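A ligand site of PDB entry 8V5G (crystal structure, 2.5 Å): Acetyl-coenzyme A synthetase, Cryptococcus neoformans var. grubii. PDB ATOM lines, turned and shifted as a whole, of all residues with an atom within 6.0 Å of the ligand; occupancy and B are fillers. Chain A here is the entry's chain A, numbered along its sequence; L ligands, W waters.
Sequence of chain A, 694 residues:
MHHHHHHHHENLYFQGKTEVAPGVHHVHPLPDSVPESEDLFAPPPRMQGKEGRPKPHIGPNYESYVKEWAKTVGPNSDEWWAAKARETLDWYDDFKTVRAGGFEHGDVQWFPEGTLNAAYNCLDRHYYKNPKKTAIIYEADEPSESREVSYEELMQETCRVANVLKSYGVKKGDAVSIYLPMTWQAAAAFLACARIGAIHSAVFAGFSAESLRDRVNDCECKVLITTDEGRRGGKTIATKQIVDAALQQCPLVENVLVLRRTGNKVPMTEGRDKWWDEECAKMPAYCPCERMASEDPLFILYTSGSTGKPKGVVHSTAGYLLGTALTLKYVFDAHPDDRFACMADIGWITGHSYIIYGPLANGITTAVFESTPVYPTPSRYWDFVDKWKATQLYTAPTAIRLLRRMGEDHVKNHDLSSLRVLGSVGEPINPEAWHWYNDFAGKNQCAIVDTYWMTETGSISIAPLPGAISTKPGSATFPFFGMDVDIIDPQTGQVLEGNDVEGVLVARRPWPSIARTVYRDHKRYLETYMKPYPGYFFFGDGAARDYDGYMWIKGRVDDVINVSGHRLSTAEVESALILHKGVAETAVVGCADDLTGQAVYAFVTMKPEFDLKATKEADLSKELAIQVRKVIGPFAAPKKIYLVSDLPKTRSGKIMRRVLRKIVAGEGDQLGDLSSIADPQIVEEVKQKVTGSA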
ATOM      1  N   ILE A 349     -12.505   0.123 -27.895  1.00  0.00           N
ATOM      2  CA  ILE A 349     -13.214  -0.909 -27.142  1.00  0.00           C
ATOM      3  C   ILE A 349     -14.048  -1.787 -28.053  1.00  0.00           C
ATOM      4  O   ILE A 349     -14.241  -2.980 -27.765  1.00  0.00           O
ATOM      5  CB  ILE A 349     -14.076  -0.292 -26.034  1.00  0.00           C
ATOM      6  CG1 ILE A 349     -14.541  -1.390 -25.061  1.00  0.00           C
ATOM      7  CG2 ILE A 349     -15.287   0.484 -26.607  1.00  0.00           C
ATOM      8  CD1 ILE A 349     -13.383  -1.955 -24.281  1.00  0.00           C
ATOM      9  N   THR A 350     -14.548  -1.252 -29.173  1.00  0.00           N
ATOM     10  CA  THR A 350     -15.323  -2.074 -30.101  1.00  0.00           C
ATOM     11  C   THR A 350     -14.454  -3.173 -30.713  1.00  0.00           C
ATOM     12  O   THR A 350     -14.899  -4.306 -30.889  1.00  0.00           O
ATOM     13  CB  THR A 350     -15.951  -1.204 -31.198  1.00  0.00           C
ATOM     14  OG1 THR A 350     -16.660  -0.126 -30.582  1.00  0.00           O
ATOM     15  CG2 THR A 350     -16.931  -1.975 -32.036  1.00  0.00           C
ATOM     16  N   SER A 424     -24.625  -1.001 -35.591  1.00  0.00           N
ATOM     17  CA  SER A 424     -24.110   0.355 -35.580  1.00  0.00           C
ATOM     18  C   SER A 424     -23.733   0.724 -34.151  1.00  0.00           C
ATOM     19  O   SER A 424     -24.536   0.528 -33.234  1.00  0.00           O
ATOM     20  CB  SER A 424     -25.156   1.323 -36.142  1.00  0.00           C
ATOM     21  OG  SER A 424     -24.669   2.661 -36.154  1.00  0.00           O
ATOM     22  N   VAL A 425     -22.523   1.260 -33.977  1.00  0.00           N
ATOM     23  CA  VAL A 425     -21.998   1.621 -32.675  1.00  0.00           C
ATOM     24  C   VAL A 425     -21.203   2.906 -32.823  1.00  0.00           C
ATOM     25  O   VAL A 425     -20.606   3.163 -33.879  1.00  0.00           O
ATOM     26  CB  VAL A 425     -21.103   0.524 -32.045  1.00  0.00           C
ATOM     27  CG1 VAL A 425     -19.967   0.156 -32.984  1.00  0.00           C
ATOM     28  CG2 VAL A 425     -20.531   0.964 -30.698  1.00  0.00           C
ATOM     29  N   GLY A 426     -21.151   3.687 -31.751  1.00  0.00           N
ATOM     30  CA  GLY A 426     -20.260   4.826 -31.705  1.00  0.00           C
ATOM     31  C   GLY A 426     -20.931   6.124 -31.321  1.00  0.00           C
ATOM     32  O   GLY A 426     -20.334   6.964 -30.663  1.00  0.00           O
ATOM     33  N   GLU A 427     -22.177   6.288 -31.739  1.00  0.00           N
ATOM     34  CA  GLU A 427     -22.933   7.518 -31.540  1.00  0.00           C
ATOM     35  C   GLU A 427     -24.361   7.277 -32.019  1.00  0.00           C
ATOM     36  O   GLU A 427     -24.651   6.211 -32.551  1.00  0.00           O
ATOM     37  CB  GLU A 427     -22.301   8.691 -32.285  1.00  0.00           C
ATOM     38  CG  GLU A 427     -22.269   8.534 -33.792  1.00  0.00           C
ATOM     39  CD  GLU A 427     -21.621   9.719 -34.514  1.00  0.00           C
ATOM     40  OE1 GLU A 427     -21.271  10.719 -33.831  1.00  0.00           O
ATOM     41  OE2 GLU A 427     -21.451   9.649 -35.739  1.00  0.00           O
ATOM     42  N   PRO A 428     -25.289   8.197 -31.791  1.00  0.00           N
ATOM     43  CA  PRO A 428     -26.631   8.021 -32.363  1.00  0.00           C
ATOM     44  C   PRO A 428     -26.534   8.005 -33.882  1.00  0.00           C
ATOM     45  O   PRO A 428     -25.758   8.766 -34.475  1.00  0.00           O
ATOM     46  CB  PRO A 428     -27.410   9.232 -31.859  1.00  0.00           C
ATOM     47  CG  PRO A 428     -26.641   9.726 -30.678  1.00  0.00           C
ATOM     48  CD  PRO A 428     -25.197   9.399 -30.951  1.00  0.00           C
ATOM     49  N   ILE A 429     -27.313   7.131 -34.502  1.00  0.00           N
ATOM     50  CA  ILE A 429     -27.382   7.024 -35.950  1.00  0.00           C
ATOM     51  C   ILE A 429     -28.607   7.779 -36.423  1.00  0.00           C
ATOM     52  O   ILE A 429     -29.737   7.505 -35.980  1.00  0.00           O
ATOM     53  CB  ILE A 429     -27.392   5.549 -36.400  1.00  0.00           C
ATOM     54  CG1 ILE A 429     -27.307   5.444 -37.932  1.00  0.00           C
ATOM     55  CG2 ILE A 429     -28.650   4.819 -35.910  1.00  0.00           C
ATOM     56  CD1 ILE A 429     -27.146   4.020 -38.422  1.00  0.00           C
ATOM     57  N   ASP A 450     -28.836  -1.344 -33.255  1.00  0.00           N
ATOM     58  CA  ASP A 450     -28.215  -0.121 -32.758  1.00  0.00           C
ATOM     59  C   ASP A 450     -27.716  -0.381 -31.342  1.00  0.00           C
ATOM     60  O   ASP A 450     -28.513  -0.466 -30.407  1.00  0.00           O
ATOM     61  CB  ASP A 450     -29.239   0.996 -32.790  1.00  0.00           C
ATOM     62  CG  ASP A 450     -28.654   2.351 -32.508  1.00  0.00           C
ATOM     63  OD1 ASP A 450     -27.428   2.456 -32.308  1.00  0.00           O
ATOM     64  OD2 ASP A 450     -29.435   3.322 -32.529  1.00  0.00           O
ATOM     65  N   THR A 451     -26.400  -0.473 -31.183  1.00  0.00           N
ATOM     66  CA  THR A 451     -25.809  -0.905 -29.928  1.00  0.00           C
ATOM     67  C   THR A 451     -25.284   0.321 -29.193  1.00  0.00           C
ATOM     68  O   THR A 451     -24.358   0.995 -29.674  1.00  0.00           O
ATOM     69  CB  THR A 451     -24.702  -1.929 -30.162  1.00  0.00           C
ATOM     70  OG1 THR A 451     -23.605  -1.329 -30.871  1.00  0.00           O
ATOM     71  CG2 THR A 451     -25.231  -3.108 -30.985  1.00  0.00           C
ATOM     72  N   TYR A 452     -25.857   0.601 -28.034  1.00  0.00           N
ATOM     73  CA  TYR A 452     -25.383   1.658 -27.162  1.00  0.00           C
ATOM     74  C   TYR A 452     -24.538   1.046 -26.058  1.00  0.00           C
ATOM     75  O   TYR A 452     -24.962   0.066 -25.426  1.00  0.00           O
ATOM     76  CB  TYR A 452     -26.537   2.460 -26.555  1.00  0.00           C
ATOM     77  CG  TYR A 452     -26.073   3.330 -25.406  1.00  0.00           C
ATOM     78  CD1 TYR A 452     -25.461   4.545 -25.628  1.00  0.00           C
ATOM     79  CD2 TYR A 452     -26.200   2.899 -24.087  1.00  0.00           C
ATOM     80  CE1 TYR A 452     -25.022   5.319 -24.586  1.00  0.00           C
ATOM     81  CE2 TYR A 452     -25.773   3.654 -23.052  1.00  0.00           C
ATOM     82  CZ  TYR A 452     -25.182   4.866 -23.297  1.00  0.00           C
ATOM     83  OH  TYR A 452     -24.741   5.620 -22.232  1.00  0.00           O
ATOM     84  N   TRP A 453     -23.357   1.594 -25.831  1.00  0.00           N
ATOM     85  CA  TRP A 453     -22.516   1.179 -24.707  1.00  0.00           C
ATOM     86  C   TRP A 453     -21.300   2.112 -24.690  1.00  0.00           C
ATOM     87  O   TRP A 453     -21.165   3.007 -25.499  1.00  0.00           O
ATOM     88  CB  TRP A 453     -22.130  -0.292 -24.788  1.00  0.00           C
ATOM     89  CG  TRP A 453     -21.457  -0.723 -26.058  1.00  0.00           C
ATOM     90  CD1 TRP A 453     -21.984  -0.685 -27.326  1.00  0.00           C
ATOM     91  CD2 TRP A 453     -20.139  -1.274 -26.194  1.00  0.00           C
ATOM     92  NE1 TRP A 453     -21.084  -1.176 -28.221  1.00  0.00           N
ATOM     93  CE2 TRP A 453     -19.938  -1.539 -27.565  1.00  0.00           C
ATOM     94  CE3 TRP A 453     -19.118  -1.558 -25.291  1.00  0.00           C
ATOM     95  CZ2 TRP A 453     -18.752  -2.053 -28.051  1.00  0.00           C
ATOM     96  CZ3 TRP A 453     -17.940  -2.087 -25.777  1.00  0.00           C
ATOM     97  CH2 TRP A 453     -17.766  -2.334 -27.151  1.00  0.00           C
ATOM     98  N   MET A 454     -20.418   1.882 -23.704  1.00  0.00           N
ATOM     99  CA  MET A 454     -19.220   2.701 -23.549  1.00  0.00           C
ATOM    100  C   MET A 454     -18.015   1.818 -23.300  1.00  0.00           C
ATOM    101  O   MET A 454     -18.146   0.647 -22.921  1.00  0.00           O
ATOM    102  CB  MET A 454     -19.338   3.683 -22.382  1.00  0.00           C
ATOM    103  CG  MET A 454     -20.657   4.373 -22.251  1.00  0.00           C
ATOM    104  SD  MET A 454     -20.627   5.514 -20.846  1.00  0.00           S
ATOM    105  CE  MET A 454     -19.488   6.759 -21.440  1.00  0.00           C
ATOM    106  N   THR A 455     -16.820   2.402 -23.486  1.00  0.00           N
ATOM    107  CA  THR A 455     -15.615   1.725 -23.053  1.00  0.00           C
ATOM    108  C   THR A 455     -15.782   1.210 -21.635  1.00  0.00           C
ATOM    109  O   THR A 455     -15.418   0.068 -21.339  1.00  0.00           O
ATOM    110  CB  THR A 455     -14.411   2.664 -23.122  1.00  0.00           C
ATOM    111  OG1 THR A 455     -14.227   3.138 -24.466  1.00  0.00           O
ATOM    112  CG2 THR A 455     -13.132   1.966 -22.638  1.00  0.00           C
ATOM    113  N   GLU A 456     -16.388   2.026 -20.756  1.00  0.00           N
ATOM    114  CA  GLU A 456     -16.515   1.721 -19.342  1.00  0.00           C
ATOM    115  C   GLU A 456     -17.562   0.654 -19.037  1.00  0.00           C
ATOM    116  O   GLU A 456     -17.557   0.129 -17.906  1.00  0.00           O
ATOM    117  CB  GLU A 456     -16.862   2.972 -18.551  1.00  0.00           C
ATOM    118  CG  GLU A 456     -15.769   4.054 -18.524  1.00  0.00           C
ATOM    119  CD  GLU A 456     -15.892   5.067 -19.665  1.00  0.00           C
ATOM    120  OE1 GLU A 456     -16.654   4.833 -20.628  1.00  0.00           O
ATOM    121  OE2 GLU A 456     -15.231   6.118 -19.598  1.00  0.00           O
ATOM    122  N   ALA A 476     -31.924   2.484 -29.712  1.00  0.00           N
ATOM    123  CA  ALA A 476     -31.301   1.256 -29.235  1.00  0.00           C
ATOM    124  C   ALA A 476     -32.316   0.298 -28.625  1.00  0.00           C
ATOM    125  O   ALA A 476     -32.084  -0.910 -28.654  1.00  0.00           O
ATOM    126  CB  ALA A 476     -30.224   1.590 -28.214  1.00  0.00           C
ATOM    127  N   PHE A 539     -23.799   7.191 -16.967  1.00  0.00           N
ATOM    128  CA  PHE A 539     -23.216   7.041 -18.293  1.00  0.00           C
ATOM    129  C   PHE A 539     -22.671   8.358 -18.840  1.00  0.00           C
ATOM    130  O   PHE A 539     -21.634   8.379 -19.512  1.00  0.00           O
ATOM    131  CB  PHE A 539     -24.266   6.505 -19.283  1.00  0.00           C
ATOM    132  CG  PHE A 539     -24.704   5.105 -19.021  1.00  0.00           C
ATOM    133  CD1 PHE A 539     -25.741   4.836 -18.154  1.00  0.00           C
ATOM    134  CD2 PHE A 539     -24.106   4.051 -19.678  1.00  0.00           C
ATOM    135  CE1 PHE A 539     -26.151   3.544 -17.914  1.00  0.00           C
ATOM    136  CE2 PHE A 539     -24.521   2.755 -19.446  1.00  0.00           C
ATOM    137  CZ  PHE A 539     -25.541   2.510 -18.564  1.00  0.00           C
ATOM    138  N   ASP A 541     -24.912  10.448 -20.683  1.00  0.00           N
ATOM    139  CA  ASP A 541     -25.716  10.620 -21.879  1.00  0.00           C
ATOM    140  C   ASP A 541     -27.130  11.035 -21.499  1.00  0.00           C
ATOM    141  O   ASP A 541     -27.690  10.547 -20.509  1.00  0.00           O
ATOM    142  CB  ASP A 541     -25.800   9.308 -22.707  1.00  0.00           C
ATOM    143  CG  ASP A 541     -24.512   8.991 -23.460  1.00  0.00           C
ATOM    144  OD1 ASP A 541     -23.945   9.920 -24.047  1.00  0.00           O
ATOM    145  OD2 ASP A 541     -24.074   7.812 -23.489  1.00  0.00           O
ATOM    146  N   ILE A 553     -31.124   7.224 -26.994  1.00  0.00           N
ATOM    147  CA  ILE A 553     -29.909   7.875 -26.525  1.00  0.00           C
ATOM    148  C   ILE A 553     -29.573   8.961 -27.548  1.00  0.00           C
ATOM    149  O   ILE A 553     -29.132   8.644 -28.649  1.00  0.00           O
ATOM    150  CB  ILE A 553     -28.740   6.888 -26.397  1.00  0.00           C
ATOM    151  CG1 ILE A 553     -29.174   5.609 -25.670  1.00  0.00           C
ATOM    152  CG2 ILE A 553     -27.562   7.598 -25.707  1.00  0.00           C
ATOM    153  CD1 ILE A 553     -29.702   5.835 -24.262  1.00  0.00           C
ATOM    154  N   LYS A 554     -29.672  10.226 -27.151  1.00  0.00           N
ATOM    155  CA  LYS A 554     -29.612  11.320 -28.104  1.00  0.00           C
ATOM    156  C   LYS A 554     -28.340  12.139 -28.027  1.00  0.00           C
ATOM    157  O   LYS A 554     -28.181  13.074 -28.821  1.00  0.00           O
ATOM    158  CB  LYS A 554     -30.842  12.230 -27.937  1.00  0.00           C
ATOM    159  CG  LYS A 554     -32.156  11.533 -28.286  1.00  0.00           C
ATOM    160  CD  LYS A 554     -33.365  12.439 -28.052  1.00  0.00           C
ATOM    161  CE  LYS A 554     -34.668  11.706 -28.364  1.00  0.00           C
ATOM    162  NZ  LYS A 554     -35.862  12.586 -28.127  1.00  0.00           N
ATOM    163  N   GLY A 555     -27.415  11.809 -27.139  1.00  0.00           N
ATOM    164  CA  GLY A 555     -26.117  12.453 -27.109  1.00  0.00           C
ATOM    165  C   GLY A 555     -25.593  12.832 -25.736  1.00  0.00           C
ATOM    166  O   GLY A 555     -26.316  12.751 -24.736  1.00  0.00           O
ATOM    167  N   ARG A 556     -24.334  13.279 -25.696  1.00  0.00           N
ATOM    168  CA  ARG A 556     -23.674  13.530 -24.432  1.00  0.00           C
ATOM    169  C   ARG A 556     -24.360  14.679 -23.709  1.00  0.00           C
ATOM    170  O   ARG A 556     -24.806  15.646 -24.335  1.00  0.00           O
ATOM    171  CB  ARG A 556     -22.193  13.848 -24.655  1.00  0.00           C
ATOM    172  CG  ARG A 556     -21.374  12.734 -25.343  1.00  0.00           C
ATOM    173  CD  ARG A 556     -21.256  11.443 -24.505  1.00  0.00           C
ATOM    174  NE  ARG A 556     -20.568  11.630 -23.228  1.00  0.00           N
ATOM    175  CZ  ARG A 556     -20.470  10.713 -22.265  1.00  0.00           C
ATOM    176  NH1 ARG A 556     -20.998   9.502 -22.383  1.00  0.00           N
ATOM    177  NH2 ARG A 556     -19.844  11.024 -21.128  1.00  0.00           N
ATOM    178  N   SER A 652     -11.141   7.840 -33.600  1.00  0.00           N
ATOM    179  CA  SER A 652     -12.168   6.902 -33.176  1.00  0.00           C
ATOM    180  C   SER A 652     -13.433   6.978 -34.013  1.00  0.00           C
ATOM    181  O   SER A 652     -14.375   6.224 -33.758  1.00  0.00           O
ATOM    182  CB  SER A 652     -12.527   7.154 -31.702  1.00  0.00           C
ATOM    183  OG  SER A 652     -13.615   6.343 -31.275  1.00  0.00           O
ATOM    184  N   LYS A 654     -15.252   9.742 -34.100  1.00  0.00           N
ATOM    185  CA  LYS A 654     -16.099  10.730 -33.446  1.00  0.00           C
ATOM    186  C   LYS A 654     -15.820  12.108 -34.023  1.00  0.00           C
ATOM    187  O   LYS A 654     -14.676  12.438 -34.347  1.00  0.00           O
ATOM    188  CB  LYS A 654     -15.872  10.703 -31.933  1.00  0.00           C
ATOM    189  CG  LYS A 654     -16.116   9.333 -31.252  1.00  0.00           C
ATOM    190  CD  LYS A 654     -17.618   8.980 -31.130  1.00  0.00           C
ATOM    191  CE  LYS A 654     -18.335   9.843 -30.066  1.00  0.00           C
ATOM    192  NZ  LYS A 654     -19.797   9.535 -29.848  1.00  0.00           N
HETATM  193  N1  LIG L   1     -25.536   3.702 -30.380  1.00  0.00           N
HETATM  194  N2  LIG L   1     -18.641   5.903 -28.476  1.00  0.00           N
HETATM  195  C1  LIG L   1     -21.971   7.066 -26.900  1.00  0.00           C
HETATM  196  C2  LIG L   1     -21.440   6.426 -25.616  1.00  0.00           C
HETATM  197  C3  LIG L   1     -19.976   6.160 -25.975  1.00  0.00           C
HETATM  198  C4  LIG L   1     -19.649   7.375 -26.833  1.00  0.00           C
HETATM  199  C5  LIG L   1     -18.518   7.199 -27.800  1.00  0.00           C
HETATM  200  C6  LIG L   1     -18.954   1.674 -27.396  1.00  0.00           C
HETATM  201  C7  LIG L   1     -25.239   4.770 -29.641  1.00  0.00           C
HETATM  202  C8  LIG L   1     -22.045   4.894 -28.206  1.00  0.00           C
HETATM  203  C9  LIG L   1     -25.957   6.816 -28.750  1.00  0.00           C
HETATM  204  C10 LIG L   1     -24.002   4.948 -29.010  1.00  0.00           C
HETATM  205  C11 LIG L   1     -23.849   6.105 -28.283  1.00  0.00           C
HETATM  206  C12 LIG L   1     -18.886   2.958 -28.134  1.00  0.00           C
HETATM  207  N3  LIG L   1     -22.587   6.065 -27.768  1.00  0.00           N
HETATM  208  N4  LIG L   1     -17.575   3.570 -28.031  1.00  0.00           N
HETATM  209  N5  LIG L   1     -22.855   4.187 -28.957  1.00  0.00           N
HETATM  210  N6  LIG L   1     -24.795   7.040 -28.142  1.00  0.00           N
HETATM  211  N7  LIG L   1     -26.192   5.727 -29.481  1.00  0.00           N
HETATM  212  O1  LIG L   1     -21.536   7.330 -24.543  1.00  0.00           O
HETATM  213  O2  LIG L   1     -19.145   6.103 -24.830  1.00  0.00           O
HETATM  214  O3  LIG L   1     -17.149   4.860 -30.098  1.00  0.00           O
HETATM  215  O4  LIG L   1     -16.283   5.629 -27.920  1.00  0.00           O
HETATM  216  O5  LIG L   1     -20.857   7.646 -27.571  1.00  0.00           O
HETATM  217  S1  LIG L   1     -17.315   5.021 -28.698  1.00  0.00           S
HETATM  218  O   HOH W   1     -24.622   9.869 -26.914  1.00  0.00           O
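The side-chain hydroxyl of Tyr 452 is in hydrogen-bond range of the side-chain carboxylate of Asp 541 (2.6 Å).
The backbone NH of Thr 451 lies within hydrogen-bond range of the backbone carbonyl oxygen of Ser 424 (2.9 Å).
NZ of Lys 654 is in hydrogen-bond range of O of Gly 426 (2.8 Å).
The guanidinium group of Arg 556 lies within hydrogen-bond range of the backbone carbonyl oxygen of Phe 539, at 3.1 Å.
The side-chain carboxylate (OD1) of Asp 541 lies within salt-bridge range of the guanidinium group (NH1) of Arg 556, at 3.4 Å.
Water W1 lies within hydrogen-bond range of the side-chain carboxylate (OD1) of Asp 541 (2.9 Å), a nitrogen (N6) of the ligand (3.1 Å) and the backbone NH (N) of Gly 555 (3.4 Å).
NZ of Lys 654 sits at hydrogen-bond distance from O5 of the ligand (3.1 Å).
A nitrogen (N1) of the ligand lies close to the backbone carbonyl oxygen of Glu 427 (3.4 Å).
An oxygen (O1) of the ligand sits at hydrogen-bond distance from the side-chain carboxylate of Asp 541, at 2.8 Å.
The backbone NH (N) of Gly 426 sits at hydrogen-bond distance from a nitrogen (N5) of the ligand, 3.3 Å away.
NH1 of Arg 556 lies within hydrogen-bond range of O1 of the ligand (3.1 Å).
O of Thr 451 lies within hydrogen-bond range of N1 of the ligand, at 3.0 Å.
O of Gly 426 is in hydrogen-bond range of N2 of the ligand (3.0 Å).
OD1 of Asp 450 is in hydrogen-bond range of N1 of the ligand, at 3.0 Å.
CG2 of Ile 349 touches C6 of the ligand, at 3.9 Å.
Val 425 touches the ligand.
N of Pro 428 touches C9 of the ligand, at 3.4 Å.
CD1 of Tyr 452 touches C11 of the ligand, 3.5 Å away.
Trp 453 touches the ligand (O to C6, 3.2 Å).
Met 454 touches the ligand.
Ile 553 touches the ligand (CG2 to C9, 3.5 Å).
Hydrophobic or aromatic side chains within 4 Å of the ligand: Ile 349, Val 425, Pro 428, Tyr 452, Trp 453, Met 454 and Ile 553.
Along chain A the residues within 4 Å of the ligand span positions 349 to 654.
The nearest printed residue that does not touch the ligand is Ser 652 (4.01 Å).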
